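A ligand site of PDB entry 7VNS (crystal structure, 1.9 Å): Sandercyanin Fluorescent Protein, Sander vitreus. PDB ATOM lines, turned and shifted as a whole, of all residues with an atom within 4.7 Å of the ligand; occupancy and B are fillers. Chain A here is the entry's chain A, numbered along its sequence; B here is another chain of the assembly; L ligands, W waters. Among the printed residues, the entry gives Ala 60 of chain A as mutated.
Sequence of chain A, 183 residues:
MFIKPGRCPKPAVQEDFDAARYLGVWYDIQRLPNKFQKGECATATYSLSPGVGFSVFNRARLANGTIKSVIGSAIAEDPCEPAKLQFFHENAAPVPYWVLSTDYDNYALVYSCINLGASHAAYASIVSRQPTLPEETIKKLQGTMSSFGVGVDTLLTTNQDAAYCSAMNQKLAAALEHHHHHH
The side-chain amide nitrogen of Asn 58 sits at hydrogen-bond distance from a nitrogen (N4) of the ligand.
An oxygen (O6) of the ligand lies within hydrogen-bond range of the backbone NH (N) of Lys 38, 3.1 Å away.
The side-chain amino group (NZ) of Lys 38 lies within salt-bridge range of an oxygen (O1) of the ligand (3.1 Å).
An oxygen (O3) of the ligand is in hydrogen-bond range of the guanidinium group of Arg 31 (2.7 Å).
The backbone carbonyl oxygen (O) of Pro 96 is in hydrogen-bond range of the side-chain hydroxyl (OG) of Ser 112 (2.5 Å).
The side-chain carboxylate (OD1) of Asp 28 is in hydrogen-bond range of the side-chain hydroxyl (OG) of Ser 125, 2.6 Å away.
The side-chain hydroxyl (OH) of Tyr 97 sits at hydrogen-bond distance from the side-chain hydroxyl (OH) of Tyr 46.
O of Ala 60 is in hydrogen-bond range of N of Lys 68, at 2.8 Å.
The backbone carbonyl oxygen of Ala 44 sits at hydrogen-bond distance from the backbone NH of Trp 26 (2.8 Å).
The backbone NH of Asp 28 sits at hydrogen-bond distance from the backbone carbonyl oxygen of Ala 42, at 2.9 Å.
O of Thr 43 is in hydrogen-bond range of N of Arg 59 (2.9 Å).
The backbone carbonyl oxygen (O) of Val 110 sits at hydrogen-bond distance from the backbone NH (N) of Ser 125 (2.9 Å).
Merely in contact with the ligand: His 89 (3.4 Å), Arg 59 (3.4 Å), Tyr 97 (3.4 Å), Pro 96 (3.4 Å), Ala 44 (3.4 Å), Tyr 123 (3.4 Å), Ala 118 of chain B (3.5 Å), Val 110 (3.6 Å), Thr 43 (3.6 Å), Val 70 (3.6 Å), Val 95 (3.6 Å), Ala 60 (3.7 Å), Asp 28 (3.8 Å), Val 127 (3.9 Å), Ser 112 (3.9 Å), Trp 26 (3.9 Å), Glu 90 (3.9 Å), Tyr 46 (3.97 Å) and Ala 42 (3.99 Å).
Hydrophobic or aromatic side chains that line the ligand: Ala 42, Ala 44, Ala 60, Val 70, His 89, Val 95, Tyr 97, Val 110, Tyr 123, Val 127 and Ala 118 of chain B.
Of the 31 residues printed, 22 come within 4 Å of the ligand.
Along chain A the residues within 4 Å of the ligand span positions 26 to 127.
Water W1 bridges an oxygen (O1) of the ligand (2.6 Å) and the side-chain amino group (NZ) of Lys 38 (2.6 Å).
Water W4 lies within hydrogen-bond range of a ring nitrogen (NE2) of His 89 (2.8 Å), an oxygen (O4) of the ligand (2.8 Å) and the side-chain amide nitrogen (ND2) of Asn 58 (2.9 Å).
Water W3 lies within hydrogen-bond range of O5 of the ligand, O of Phe 36 and NZ of Lys 38.
Water W6 lies within hydrogen-bond range of OH of Tyr 46 (2.7 Å), OD1 of Asn 58 (2.8 Å) and O4 of the ligand (3.2 Å).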
ATOM      1  N   TRP A  26     -15.942   7.104  15.050  1.00  0.00           N
ATOM      2  CA  TRP A  26     -14.883   7.594  14.151  1.00  0.00           C
ATOM      3  C   TRP A  26     -13.777   6.530  14.094  1.00  0.00           C
ATOM      4  O   TRP A  26     -13.392   5.989  15.142  1.00  0.00           O
ATOM      5  CB  TRP A  26     -14.327   8.939  14.605  1.00  0.00           C
ATOM      6  CG  TRP A  26     -15.266  10.099  14.495  1.00  0.00           C
ATOM      7  CD1 TRP A  26     -16.060  10.606  15.466  1.00  0.00           C
ATOM      8  CD2 TRP A  26     -15.535  10.866  13.314  1.00  0.00           C
ATOM      9  NE1 TRP A  26     -16.757  11.694  15.008  1.00  0.00           N
ATOM     10  CE2 TRP A  26     -16.458  11.879  13.667  1.00  0.00           C
ATOM     11  CE3 TRP A  26     -15.046  10.846  12.004  1.00  0.00           C
ATOM     12  CZ2 TRP A  26     -16.908  12.817  12.740  1.00  0.00           C
ATOM     13  CZ3 TRP A  26     -15.485  11.774  11.105  1.00  0.00           C
ATOM     14  CH2 TRP A  26     -16.384  12.772  11.464  1.00  0.00           C
ATOM     15  N   TYR A  27     -13.243   6.305  12.903  1.00  0.00           N
ATOM     16  CA  TYR A  27     -12.126   5.344  12.640  1.00  0.00           C
ATOM     17  C   TYR A  27     -10.847   6.147  12.450  1.00  0.00           C
ATOM     18  O   TYR A  27     -10.813   7.076  11.662  1.00  0.00           O
ATOM     19  CB  TYR A  27     -12.329   4.475  11.399  1.00  0.00           C
ATOM     20  CG  TYR A  27     -13.493   3.540  11.532  1.00  0.00           C
ATOM     21  CD1 TYR A  27     -14.785   3.984  11.242  1.00  0.00           C
ATOM     22  CD2 TYR A  27     -13.333   2.238  11.977  1.00  0.00           C
ATOM     23  CE1 TYR A  27     -15.889   3.161  11.406  1.00  0.00           C
ATOM     24  CE2 TYR A  27     -14.431   1.411  12.173  1.00  0.00           C
ATOM     25  CZ  TYR A  27     -15.701   1.877  11.882  1.00  0.00           C
ATOM     26  OH  TYR A  27     -16.783   1.091  12.046  1.00  0.00           O
ATOM     27  N   ASP A  28      -9.790   5.710  13.101  1.00  0.00           N
ATOM     28  CA  ASP A  28      -8.449   6.328  12.923  1.00  0.00           C
ATOM     29  C   ASP A  28      -7.896   5.933  11.543  1.00  0.00           C
ATOM     30  O   ASP A  28      -7.783   4.728  11.284  1.00  0.00           O
ATOM     31  CB  ASP A  28      -7.559   5.884  14.057  1.00  0.00           C
ATOM     32  CG  ASP A  28      -6.357   6.804  14.177  1.00  0.00           C
ATOM     33  OD1 ASP A  28      -6.557   8.055  14.330  1.00  0.00           O
ATOM     34  OD2 ASP A  28      -5.284   6.310  14.052  1.00  0.00           O
ATOM     35  N   ARG A  31      -2.156   9.149  11.498  1.00  0.00           N
ATOM     36  CA  ARG A  31      -1.812   9.981  12.674  1.00  0.00           C
ATOM     37  C   ARG A  31      -0.305  10.150  12.776  1.00  0.00           C
ATOM     38  O   ARG A  31       0.436   9.393  12.087  1.00  0.00           O
ATOM     39  CB  ARG A  31      -2.421   9.371  13.920  1.00  0.00           C
ATOM     40  CG  ARG A  31      -1.905   7.991  14.268  1.00  0.00           C
ATOM     41  CD  ARG A  31      -2.231   7.729  15.718  1.00  0.00           C
ATOM     42  NE  ARG A  31      -3.655   7.895  16.044  1.00  0.00           N
ATOM     43  CZ  ARG A  31      -4.165   8.797  16.893  1.00  0.00           C
ATOM     44  NH1 ARG A  31      -3.365   9.666  17.509  1.00  0.00           N
ATOM     45  NH2 ARG A  31      -5.485   8.833  17.084  1.00  0.00           N
ATOM     46  N   PHE A  36       3.788   5.585  22.708  1.00  0.00           N
ATOM     47  CA  PHE A  36       3.018   4.696  23.623  1.00  0.00           C
ATOM     48  C   PHE A  36       1.662   4.289  22.988  1.00  0.00           C
ATOM     49  O   PHE A  36       0.786   3.765  23.683  1.00  0.00           O
ATOM     50  CB  PHE A  36       2.902   5.346  25.004  1.00  0.00           C
ATOM     51  CG  PHE A  36       4.230   5.726  25.619  1.00  0.00           C
ATOM     52  CD1 PHE A  36       5.185   4.750  25.920  1.00  0.00           C
ATOM     53  CD2 PHE A  36       4.564   7.048  25.847  1.00  0.00           C
ATOM     54  CE1 PHE A  36       6.405   5.100  26.462  1.00  0.00           C
ATOM     55  CE2 PHE A  36       5.796   7.400  26.380  1.00  0.00           C
ATOM     56  CZ  PHE A  36       6.716   6.423  26.681  1.00  0.00           C
ATOM     57  N   GLN A  37       1.503   4.525  21.691  1.00  0.00           N
ATOM     58  CA  GLN A  37       0.361   3.979  20.905  1.00  0.00           C
ATOM     59  C   GLN A  37       0.274   2.486  21.210  1.00  0.00           C
ATOM     60  O   GLN A  37       1.278   1.812  21.030  1.00  0.00           O
ATOM     61  CB  GLN A  37       0.502   4.087  19.385  1.00  0.00           C
ATOM     62  CG  GLN A  37      -0.551   3.261  18.644  1.00  0.00           C
ATOM     63  CD  GLN A  37      -0.809   3.743  17.232  1.00  0.00           C
ATOM     64  OE1 GLN A  37      -0.609   4.913  16.914  1.00  0.00           O
ATOM     65  NE2 GLN A  37      -1.253   2.833  16.387  1.00  0.00           N
ATOM     66  N   LYS A  38      -0.881   2.062  21.717  1.00  0.00           N
ATOM     67  CA  LYS A  38      -1.285   0.652  21.787  1.00  0.00           C
ATOM     68  C   LYS A  38      -2.277   0.455  20.625  1.00  0.00           C
ATOM     69  O   LYS A  38      -3.264   1.289  20.429  1.00  0.00           O
ATOM     70  CB  LYS A  38      -1.829   0.332  23.188  1.00  0.00           C
ATOM     71  CG  LYS A  38      -1.032   0.894  24.351  1.00  0.00           C
ATOM     72  CD  LYS A  38      -1.887   1.215  25.555  1.00  0.00           C
ATOM     73  CE  LYS A  38      -1.102   1.752  26.736  1.00  0.00           C
ATOM     74  NZ  LYS A  38      -1.198   3.228  26.826  1.00  0.00           N
ATOM     75  N   ALA A  42      -7.955   1.442  15.522  1.00  0.00           N
ATOM     76  CA  ALA A  42      -8.427   2.354  16.590  1.00  0.00           C
ATOM     77  C   ALA A  42      -9.735   3.025  16.126  1.00  0.00           C
ATOM     78  O   ALA A  42      -9.839   3.466  14.981  1.00  0.00           O
ATOM     79  CB  ALA A  42      -7.357   3.366  16.922  1.00  0.00           C
ATOM     80  N   THR A  43     -10.705   3.059  17.027  1.00  0.00           N
ATOM     81  CA  THR A  43     -11.940   3.844  16.939  1.00  0.00           C
ATOM     82  C   THR A  43     -12.129   4.700  18.184  1.00  0.00           C
ATOM     83  O   THR A  43     -11.676   4.350  19.313  1.00  0.00           O
ATOM     84  CB  THR A  43     -13.177   2.951  16.760  1.00  0.00           C
ATOM     85  OG1 THR A  43     -13.336   2.198  17.947  1.00  0.00           O
ATOM     86  CG2 THR A  43     -13.096   2.033  15.585  1.00  0.00           C
ATOM     87  N   ALA A  44     -12.852   5.788  17.963  1.00  0.00           N
ATOM     88  CA  ALA A  44     -13.307   6.748  18.988  1.00  0.00           C
ATOM     89  C   ALA A  44     -14.837   6.755  18.895  1.00  0.00           C
ATOM     90  O   ALA A  44     -15.355   6.909  17.778  1.00  0.00           O
ATOM     91  CB  ALA A  44     -12.698   8.112  18.758  1.00  0.00           C
ATOM     92  N   TYR A  46     -18.057   8.760  20.546  1.00  0.00           N
ATOM     93  CA  TYR A  46     -18.481   9.913  21.335  1.00  0.00           C
ATOM     94  C   TYR A  46     -19.988   9.795  21.580  1.00  0.00           C
ATOM     95  O   TYR A  46     -20.733   9.566  20.622  1.00  0.00           O
ATOM     96  CB  TYR A  46     -18.094  11.187  20.615  1.00  0.00           C
ATOM     97  CG  TYR A  46     -16.626  11.283  20.309  1.00  0.00           C
ATOM     98  CD1 TYR A  46     -15.669  10.977  21.263  1.00  0.00           C
ATOM     99  CD2 TYR A  46     -16.185  11.683  19.049  1.00  0.00           C
ATOM    100  CE1 TYR A  46     -14.310  11.042  20.944  1.00  0.00           C
ATOM    101  CE2 TYR A  46     -14.838  11.775  18.742  1.00  0.00           C
ATOM    102  CZ  TYR A  46     -13.897  11.418  19.701  1.00  0.00           C
ATOM    103  OH  TYR A  46     -12.578  11.497  19.376  1.00  0.00           O
ATOM    104  N   ASN A  58     -12.748   4.994  23.588  1.00  0.00           N
ATOM    105  CA  ASN A  58     -11.768   4.681  22.530  1.00  0.00           C
ATOM    106  C   ASN A  58     -11.426   3.197  22.634  1.00  0.00           C
ATOM    107  O   ASN A  58     -11.314   2.680  23.765  1.00  0.00           O
ATOM    108  CB  ASN A  58     -10.493   5.480  22.674  1.00  0.00           C
ATOM    109  CG  ASN A  58     -10.704   6.971  22.600  1.00  0.00           C
ATOM    110  OD1 ASN A  58     -11.640   7.446  21.968  1.00  0.00           O
ATOM    111  ND2 ASN A  58      -9.808   7.699  23.234  1.00  0.00           N
ATOM    112  N   ARG A  59     -11.260   2.542  21.488  1.00  0.00           N
ATOM    113  CA  ARG A  59     -10.975   1.097  21.427  1.00  0.00           C
ATOM    114  C   ARG A  59      -9.853   0.840  20.410  1.00  0.00           C
ATOM    115  O   ARG A  59      -9.853   1.482  19.336  1.00  0.00           O
ATOM    116  CB  ARG A  59     -12.224   0.322  20.975  1.00  0.00           C
ATOM    117  CG  ARG A  59     -13.413   0.524  21.898  1.00  0.00           C
ATOM    118  CD  ARG A  59     -14.687  -0.129  21.378  1.00  0.00           C
ATOM    119  NE  ARG A  59     -14.641  -1.580  21.545  1.00  0.00           N
ATOM    120  CZ  ARG A  59     -14.846  -2.484  20.596  1.00  0.00           C
ATOM    121  NH1 ARG A  59     -15.098  -2.107  19.352  1.00  0.00           N
ATOM    122  NH2 ARG A  59     -14.766  -3.772  20.902  1.00  0.00           N
ATOM    123  N   ALA A  60      -8.968  -0.096  20.716  1.00  0.00           N
ATOM    124  CA  ALA A  60      -7.933  -0.531  19.742  1.00  0.00           C
ATOM    125  C   ALA A  60      -7.677  -2.046  19.903  1.00  0.00           C
ATOM    126  O   ALA A  60      -7.951  -2.590  20.983  1.00  0.00           O
ATOM    127  CB  ALA A  60      -6.653   0.246  19.940  1.00  0.00           C
ATOM    128  N   LYS A  68      -8.174  -3.149  23.739  1.00  0.00           N
ATOM    129  CA  LYS A  68      -7.879  -2.176  24.792  1.00  0.00           C
ATOM    130  C   LYS A  68      -8.910  -1.060  24.667  1.00  0.00           C
ATOM    131  O   LYS A  68      -9.137  -0.578  23.563  1.00  0.00           O
ATOM    132  CB  LYS A  68      -6.472  -1.620  24.610  1.00  0.00           C
ATOM    133  CG  LYS A  68      -6.046  -0.608  25.673  1.00  0.00           C
ATOM    134  CD  LYS A  68      -6.170  -1.079  27.071  1.00  0.00           C
ATOM    135  CE  LYS A  68      -5.802  -0.015  28.094  1.00  0.00           C
ATOM    136  NZ  LYS A  68      -4.506   0.613  27.765  1.00  0.00           N
ATOM    137  N   VAL A  70     -10.424   2.771  26.555  1.00  0.00           N
ATOM    138  CA  VAL A  70     -10.247   3.855  27.542  1.00  0.00           C
ATOM    139  C   VAL A  70     -11.531   4.691  27.554  1.00  0.00           C
ATOM    140  O   VAL A  70     -12.116   4.974  26.473  1.00  0.00           O
ATOM    141  CB  VAL A  70      -9.004   4.725  27.262  1.00  0.00           C
ATOM    142  CG1 VAL A  70      -9.077   5.370  25.908  1.00  0.00           C
ATOM    143  CG2 VAL A  70      -8.851   5.809  28.302  1.00  0.00           C
ATOM    144  N   HIS A  89      -9.145  11.716  30.301  1.00  0.00           N
ATOM    145  CA  HIS A  89      -9.136  10.235  30.234  1.00  0.00           C
ATOM    146  C   HIS A  89      -8.840   9.667  31.599  1.00  0.00           C
ATOM    147  O   HIS A  89      -8.111  10.307  32.389  1.00  0.00           O
ATOM    148  CB  HIS A  89      -8.138   9.698  29.203  1.00  0.00           C
ATOM    149  CG  HIS A  89      -8.294  10.242  27.836  1.00  0.00           C
ATOM    150  ND1 HIS A  89      -7.654  11.408  27.430  1.00  0.00           N
ATOM    151  CD2 HIS A  89      -8.926   9.762  26.750  1.00  0.00           C
ATOM    152  CE1 HIS A  89      -7.911  11.618  26.150  1.00  0.00           C
ATOM    153  NE2 HIS A  89      -8.679  10.614  25.707  1.00  0.00           N
ATOM    154  N   GLU A  90      -9.369   8.479  31.863  1.00  0.00           N
ATOM    155  CA  GLU A  90      -9.120   7.787  33.127  1.00  0.00           C
ATOM    156  C   GLU A  90      -7.583   7.722  33.283  1.00  0.00           C
ATOM    157  O   GLU A  90      -6.893   7.410  32.318  1.00  0.00           O
ATOM    158  CB  GLU A  90      -9.725   6.384  33.019  1.00  0.00           C
ATOM    159  CG  GLU A  90     -10.677   6.101  34.133  1.00  0.00           C
ATOM    160  CD  GLU A  90     -11.062   4.632  34.221  1.00  0.00           C
ATOM    161  OE1 GLU A  90     -11.175   3.965  33.157  1.00  0.00           O
ATOM    162  OE2 GLU A  90     -11.194   4.155  35.367  1.00  0.00           O
ATOM    163  N   ALA A  92      -5.210   9.827  32.971  1.00  0.00           N
ATOM    164  CA  ALA A  92      -4.410  10.823  32.242  1.00  0.00           C
ATOM    165  C   ALA A  92      -4.723  12.215  32.793  1.00  0.00           C
ATOM    166  O   ALA A  92      -5.862  12.494  33.200  1.00  0.00           O
ATOM    167  CB  ALA A  92      -4.686  10.751  30.751  1.00  0.00           C
ATOM    168  N   VAL A  95      -5.721  16.857  28.356  1.00  0.00           N
ATOM    169  CA  VAL A  95      -5.057  17.166  27.078  1.00  0.00           C
ATOM    170  C   VAL A  95      -6.056  17.911  26.198  1.00  0.00           C
ATOM    171  O   VAL A  95      -7.257  17.669  26.242  1.00  0.00           O
ATOM    172  CB  VAL A  95      -4.515  15.895  26.403  1.00  0.00           C
ATOM    173  CG1 VAL A  95      -3.585  15.142  27.332  1.00  0.00           C
ATOM    174  CG2 VAL A  95      -5.633  14.974  26.017  1.00  0.00           C
ATOM    175  N   PRO A  96      -5.584  18.855  25.398  1.00  0.00           N
ATOM    176  CA  PRO A  96      -6.431  19.563  24.445  1.00  0.00           C
ATOM    177  C   PRO A  96      -6.807  18.658  23.284  1.00  0.00           C
ATOM    178  O   PRO A  96      -6.106  17.697  22.981  1.00  0.00           O
ATOM    179  CB  PRO A  96      -5.600  20.765  23.958  1.00  0.00           C
ATOM    180  CG  PRO A  96      -4.202  20.430  24.320  1.00  0.00           C
ATOM    181  CD  PRO A  96      -4.225  19.396  25.445  1.00  0.00           C
ATOM    182  N   TYR A  97      -7.919  18.999  22.650  1.00  0.00           N
ATOM    183  CA  TYR A  97      -8.451  18.260  21.492  1.00  0.00           C
ATOM    184  C   TYR A  97      -9.141  19.302  20.646  1.00  0.00           C
ATOM    185  O   TYR A  97     -10.178  19.831  21.080  1.00  0.00           O
ATOM    186  CB  TYR A  97      -9.406  17.169  21.966  1.00  0.00           C
ATOM    187  CG  TYR A  97     -10.027  16.287  20.905  1.00  0.00           C
ATOM    188  CD1 TYR A  97     -11.064  16.728  20.107  1.00  0.00           C
ATOM    189  CD2 TYR A  97      -9.668  14.953  20.768  1.00  0.00           C
ATOM    190  CE1 TYR A  97     -11.759  15.914  19.239  1.00  0.00           C
ATOM    191  CE2 TYR A  97     -10.327  14.114  19.873  1.00  0.00           C
ATOM    192  CZ  TYR A  97     -11.383  14.595  19.104  1.00  0.00           C
ATOM    193  OH  TYR A  97     -12.107  13.798  18.258  1.00  0.00           O
ATOM    194  N   VAL A 110      -8.160  16.298  13.692  1.00  0.00           N
ATOM    195  CA  VAL A 110      -8.054  16.650  15.121  1.00  0.00           C
ATOM    196  C   VAL A 110      -6.591  16.876  15.444  1.00  0.00           C
ATOM    197  O   VAL A 110      -5.726  16.153  14.928  1.00  0.00           O
ATOM    198  CB  VAL A 110      -8.654  15.507  15.941  1.00  0.00           C
ATOM    199  CG1 VAL A 110      -8.535  15.818  17.419  1.00  0.00           C
ATOM    200  CG2 VAL A 110     -10.112  15.372  15.564  1.00  0.00           C
ATOM    201  N   TYR A 111      -6.334  17.833  16.326  1.00  0.00           N
ATOM    202  CA  TYR A 111      -4.970  18.235  16.710  1.00  0.00           C
ATOM    203  C   TYR A 111      -4.944  18.524  18.225  1.00  0.00           C
ATOM    204  O   TYR A 111      -5.936  19.049  18.761  1.00  0.00           O
ATOM    205  CB  TYR A 111      -4.562  19.431  15.870  1.00  0.00           C
ATOM    206  CG  TYR A 111      -3.158  19.901  16.172  1.00  0.00           C
ATOM    207  CD1 TYR A 111      -2.080  19.126  15.783  1.00  0.00           C
ATOM    208  CD2 TYR A 111      -2.900  21.094  16.807  1.00  0.00           C
ATOM    209  CE1 TYR A 111      -0.778  19.542  16.028  1.00  0.00           C
ATOM    210  CE2 TYR A 111      -1.599  21.524  17.054  1.00  0.00           C
ATOM    211  CZ  TYR A 111      -0.537  20.734  16.663  1.00  0.00           C
ATOM    212  OH  TYR A 111       0.749  21.114  16.916  1.00  0.00           O
ATOM    213  N   SER A 112      -3.854  18.152  18.871  1.00  0.00           N
ATOM    214  CA  SER A 112      -3.616  18.332  20.338  1.00  0.00           C
ATOM    215  C   SER A 112      -2.149  18.680  20.486  1.00  0.00           C
ATOM    216  O   SER A 112      -1.341  17.908  19.943  1.00  0.00           O
ATOM    217  CB  SER A 112      -3.912  17.091  21.108  1.00  0.00           C
ATOM    218  OG  SER A 112      -3.655  17.213  22.531  1.00  0.00           O
ATOM    219  N   TYR A 123      -0.437  15.333  19.242  1.00  0.00           N
ATOM    220  CA  TYR A 123      -1.172  14.283  18.489  1.00  0.00           C
ATOM    221  C   TYR A 123      -1.779  14.972  17.280  1.00  0.00           C
ATOM    222  O   TYR A 123      -2.197  16.174  17.372  1.00  0.00           O
ATOM    223  CB  TYR A 123      -2.373  13.746  19.274  1.00  0.00           C
ATOM    224  CG  TYR A 123      -2.075  12.951  20.505  1.00  0.00           C
ATOM    225  CD1 TYR A 123      -1.665  11.631  20.395  1.00  0.00           C
ATOM    226  CD2 TYR A 123      -2.312  13.456  21.760  1.00  0.00           C
ATOM    227  CE1 TYR A 123      -1.430  10.854  21.524  1.00  0.00           C
ATOM    228  CE2 TYR A 123      -2.094  12.684  22.903  1.00  0.00           C
ATOM    229  CZ  TYR A 123      -1.667  11.373  22.781  1.00  0.00           C
ATOM    230  OH  TYR A 123      -1.466  10.584  23.885  1.00  0.00           O
ATOM    231  N   ALA A 124      -1.891  14.289  16.177  1.00  0.00           N
ATOM    232  CA  ALA A 124      -2.690  14.802  15.023  1.00  0.00           C
ATOM    233  C   ALA A 124      -3.288  13.593  14.318  1.00  0.00           C
ATOM    234  O   ALA A 124      -2.535  12.608  14.111  1.00  0.00           O
ATOM    235  CB  ALA A 124      -1.872  15.631  14.081  1.00  0.00           C
ATOM    236  N   SER A 125      -4.585  13.607  14.051  1.00  0.00           N
ATOM    237  CA  SER A 125      -5.255  12.409  13.531  1.00  0.00           C
ATOM    238  C   SER A 125      -6.230  12.805  12.416  1.00  0.00           C
ATOM    239  O   SER A 125      -6.983  13.802  12.587  1.00  0.00           O
ATOM    240  CB  SER A 125      -5.905  11.702  14.625  1.00  0.00           C
ATOM    241  OG  SER A 125      -6.677  10.643  14.105  1.00  0.00           O
ATOM    242  N   VAL A 127      -9.515  11.185  10.830  1.00  0.00           N
ATOM    243  CA  VAL A 127     -10.505  10.144  11.174  1.00  0.00           C
ATOM    244  C   VAL A 127     -11.613  10.144  10.125  1.00  0.00           C
ATOM    245  O   VAL A 127     -11.749  11.117   9.398  1.00  0.00           O
ATOM    246  CB  VAL A 127     -11.074  10.314  12.580  1.00  0.00           C
ATOM    247  CG1 VAL A 127      -9.982  10.079  13.629  1.00  0.00           C
ATOM    248  CG2 VAL A 127     -11.752  11.673  12.783  1.00  0.00           C
ATOM    249  N   GLY B 117      -0.712  13.823  29.026  1.00  0.00           N
ATOM    250  CA  GLY B 117      -1.783  12.839  29.174  1.00  0.00           C
ATOM    251  C   GLY B 117      -1.412  11.807  30.209  1.00  0.00           C
ATOM    252  O   GLY B 117      -1.343  12.120  31.415  1.00  0.00           O
ATOM    253  N   ALA B 118      -1.106  10.594  29.765  1.00  0.00           N
ATOM    254  CA  ALA B 118      -0.749   9.492  30.667  1.00  0.00           C
ATOM    255  C   ALA B 118       0.778   9.385  30.765  1.00  0.00           C
ATOM    256  O   ALA B 118       1.238   8.547  31.572  1.00  0.00           O
ATOM    257  CB  ALA B 118      -1.376   8.204  30.195  1.00  0.00           C
HETATM  258  C1  LIG L   1      -5.849   6.802  24.358  1.00  0.00           C
HETATM  259  N1  LIG L   1      -5.687   9.190  23.795  1.00  0.00           N
HETATM  260  C2  LIG L   1      -5.551   8.148  24.674  1.00  0.00           C
HETATM  261  C3  LIG L   1      -5.050   8.701  25.896  1.00  0.00           C
HETATM  262  C4  LIG L   1      -4.873  10.050  25.685  1.00  0.00           C
HETATM  263  C5  LIG L   1      -5.318  10.380  24.364  1.00  0.00           C
HETATM  264  C6  LIG L   1      -4.377  11.066  26.663  1.00  0.00           C
HETATM  265  C7  LIG L   1      -4.817   7.948  27.176  1.00  0.00           C
HETATM  266  C8  LIG L   1      -3.752   6.870  27.170  1.00  0.00           C
HETATM  267  C9  LIG L   1      -3.724   6.019  28.450  1.00  0.00           C
HETATM  268  O1  LIG L   1      -2.672   5.350  28.591  1.00  0.00           O
HETATM  269  O2  LIG L   1      -4.706   6.063  29.323  1.00  0.00           O
HETATM  270  C10 LIG L   1      -5.341  11.590  23.716  1.00  0.00           C
HETATM  271  N2  LIG L   1      -5.306  10.920  21.411  1.00  0.00           N
HETATM  272  C11 LIG L   1      -5.489  11.844  22.389  1.00  0.00           C
HETATM  273  C12 LIG L   1      -5.830  13.068  21.781  1.00  0.00           C
HETATM  274  C13 LIG L   1      -5.741  12.922  20.407  1.00  0.00           C
HETATM  275  C14 LIG L   1      -5.379  11.513  20.187  1.00  0.00           C
HETATM  276  C15 LIG L   1      -6.238  14.301  22.506  1.00  0.00           C
HETATM  277  O3  LIG L   1      -5.176  10.906  19.128  1.00  0.00           O
HETATM  278  C16 LIG L   1      -5.974  13.961  19.473  1.00  0.00           C
HETATM  279  C17 LIG L   1      -5.646  13.886  18.221  1.00  0.00           C
HETATM  280  N3  LIG L   1      -7.948   9.007  20.412  1.00  0.00           N
HETATM  281  C18 LIG L   1      -8.402  10.153  19.765  1.00  0.00           C
HETATM  282  C19 LIG L   1      -8.779   9.764  18.399  1.00  0.00           C
HETATM  283  C20 LIG L   1      -8.651   8.371  18.344  1.00  0.00           C
HETATM  284  C21 LIG L   1      -8.114   7.898  19.574  1.00  0.00           C
HETATM  285  C22 LIG L   1      -9.241  10.752  17.351  1.00  0.00           C
HETATM  286  O4  LIG L   1      -8.463  11.278  20.237  1.00  0.00           O
HETATM  287  C23 LIG L   1      -8.891   7.500  17.287  1.00  0.00           C
HETATM  288  C24 LIG L   1      -9.979   7.195  16.708  1.00  0.00           C
HETATM  289  C25 LIG L   1      -7.816   6.634  19.914  1.00  0.00           C
HETATM  290  N4  LIG L   1      -6.831   7.077  22.109  1.00  0.00           N
HETATM  291  C26 LIG L   1      -7.361   6.227  21.160  1.00  0.00           C
HETATM  292  C27 LIG L   1      -7.310   4.875  21.639  1.00  0.00           C
HETATM  293  C28 LIG L   1      -6.806   4.909  22.905  1.00  0.00           C
HETATM  294  C29 LIG L   1      -6.445   6.292  23.169  1.00  0.00           C
HETATM  295  C30 LIG L   1      -7.727   3.634  20.890  1.00  0.00           C
HETATM  296  C31 LIG L   1      -6.592   3.759  23.817  1.00  0.00           C
HETATM  297  C32 LIG L   1      -5.423   2.896  23.344  1.00  0.00           C
HETATM  298  C33 LIG L   1      -4.094   3.567  23.559  1.00  0.00           C
HETATM  299  O5  LIG L   1      -3.833   3.886  24.705  1.00  0.00           O
HETATM  300  O6  LIG L   1      -3.337   3.772  22.574  1.00  0.00           O
HETATM  301  O   HOH W   1      -0.576   5.740  27.129  1.00  0.00           O
HETATM  302  O   HOH W   2      -4.128   8.111  21.009  1.00  0.00           O
HETATM  303  O   HOH W   3      -1.488   5.456  24.275  1.00  0.00           O
HETATM  304  O   HOH W   4      -8.774  10.393  22.900  1.00  0.00           O
HETATM  305  O   HOH W   5      -3.767   5.659  19.927  1.00  0.00           O
HETATM  306  O   HOH W   6     -11.260  10.128  21.269  1.00  0.00           O
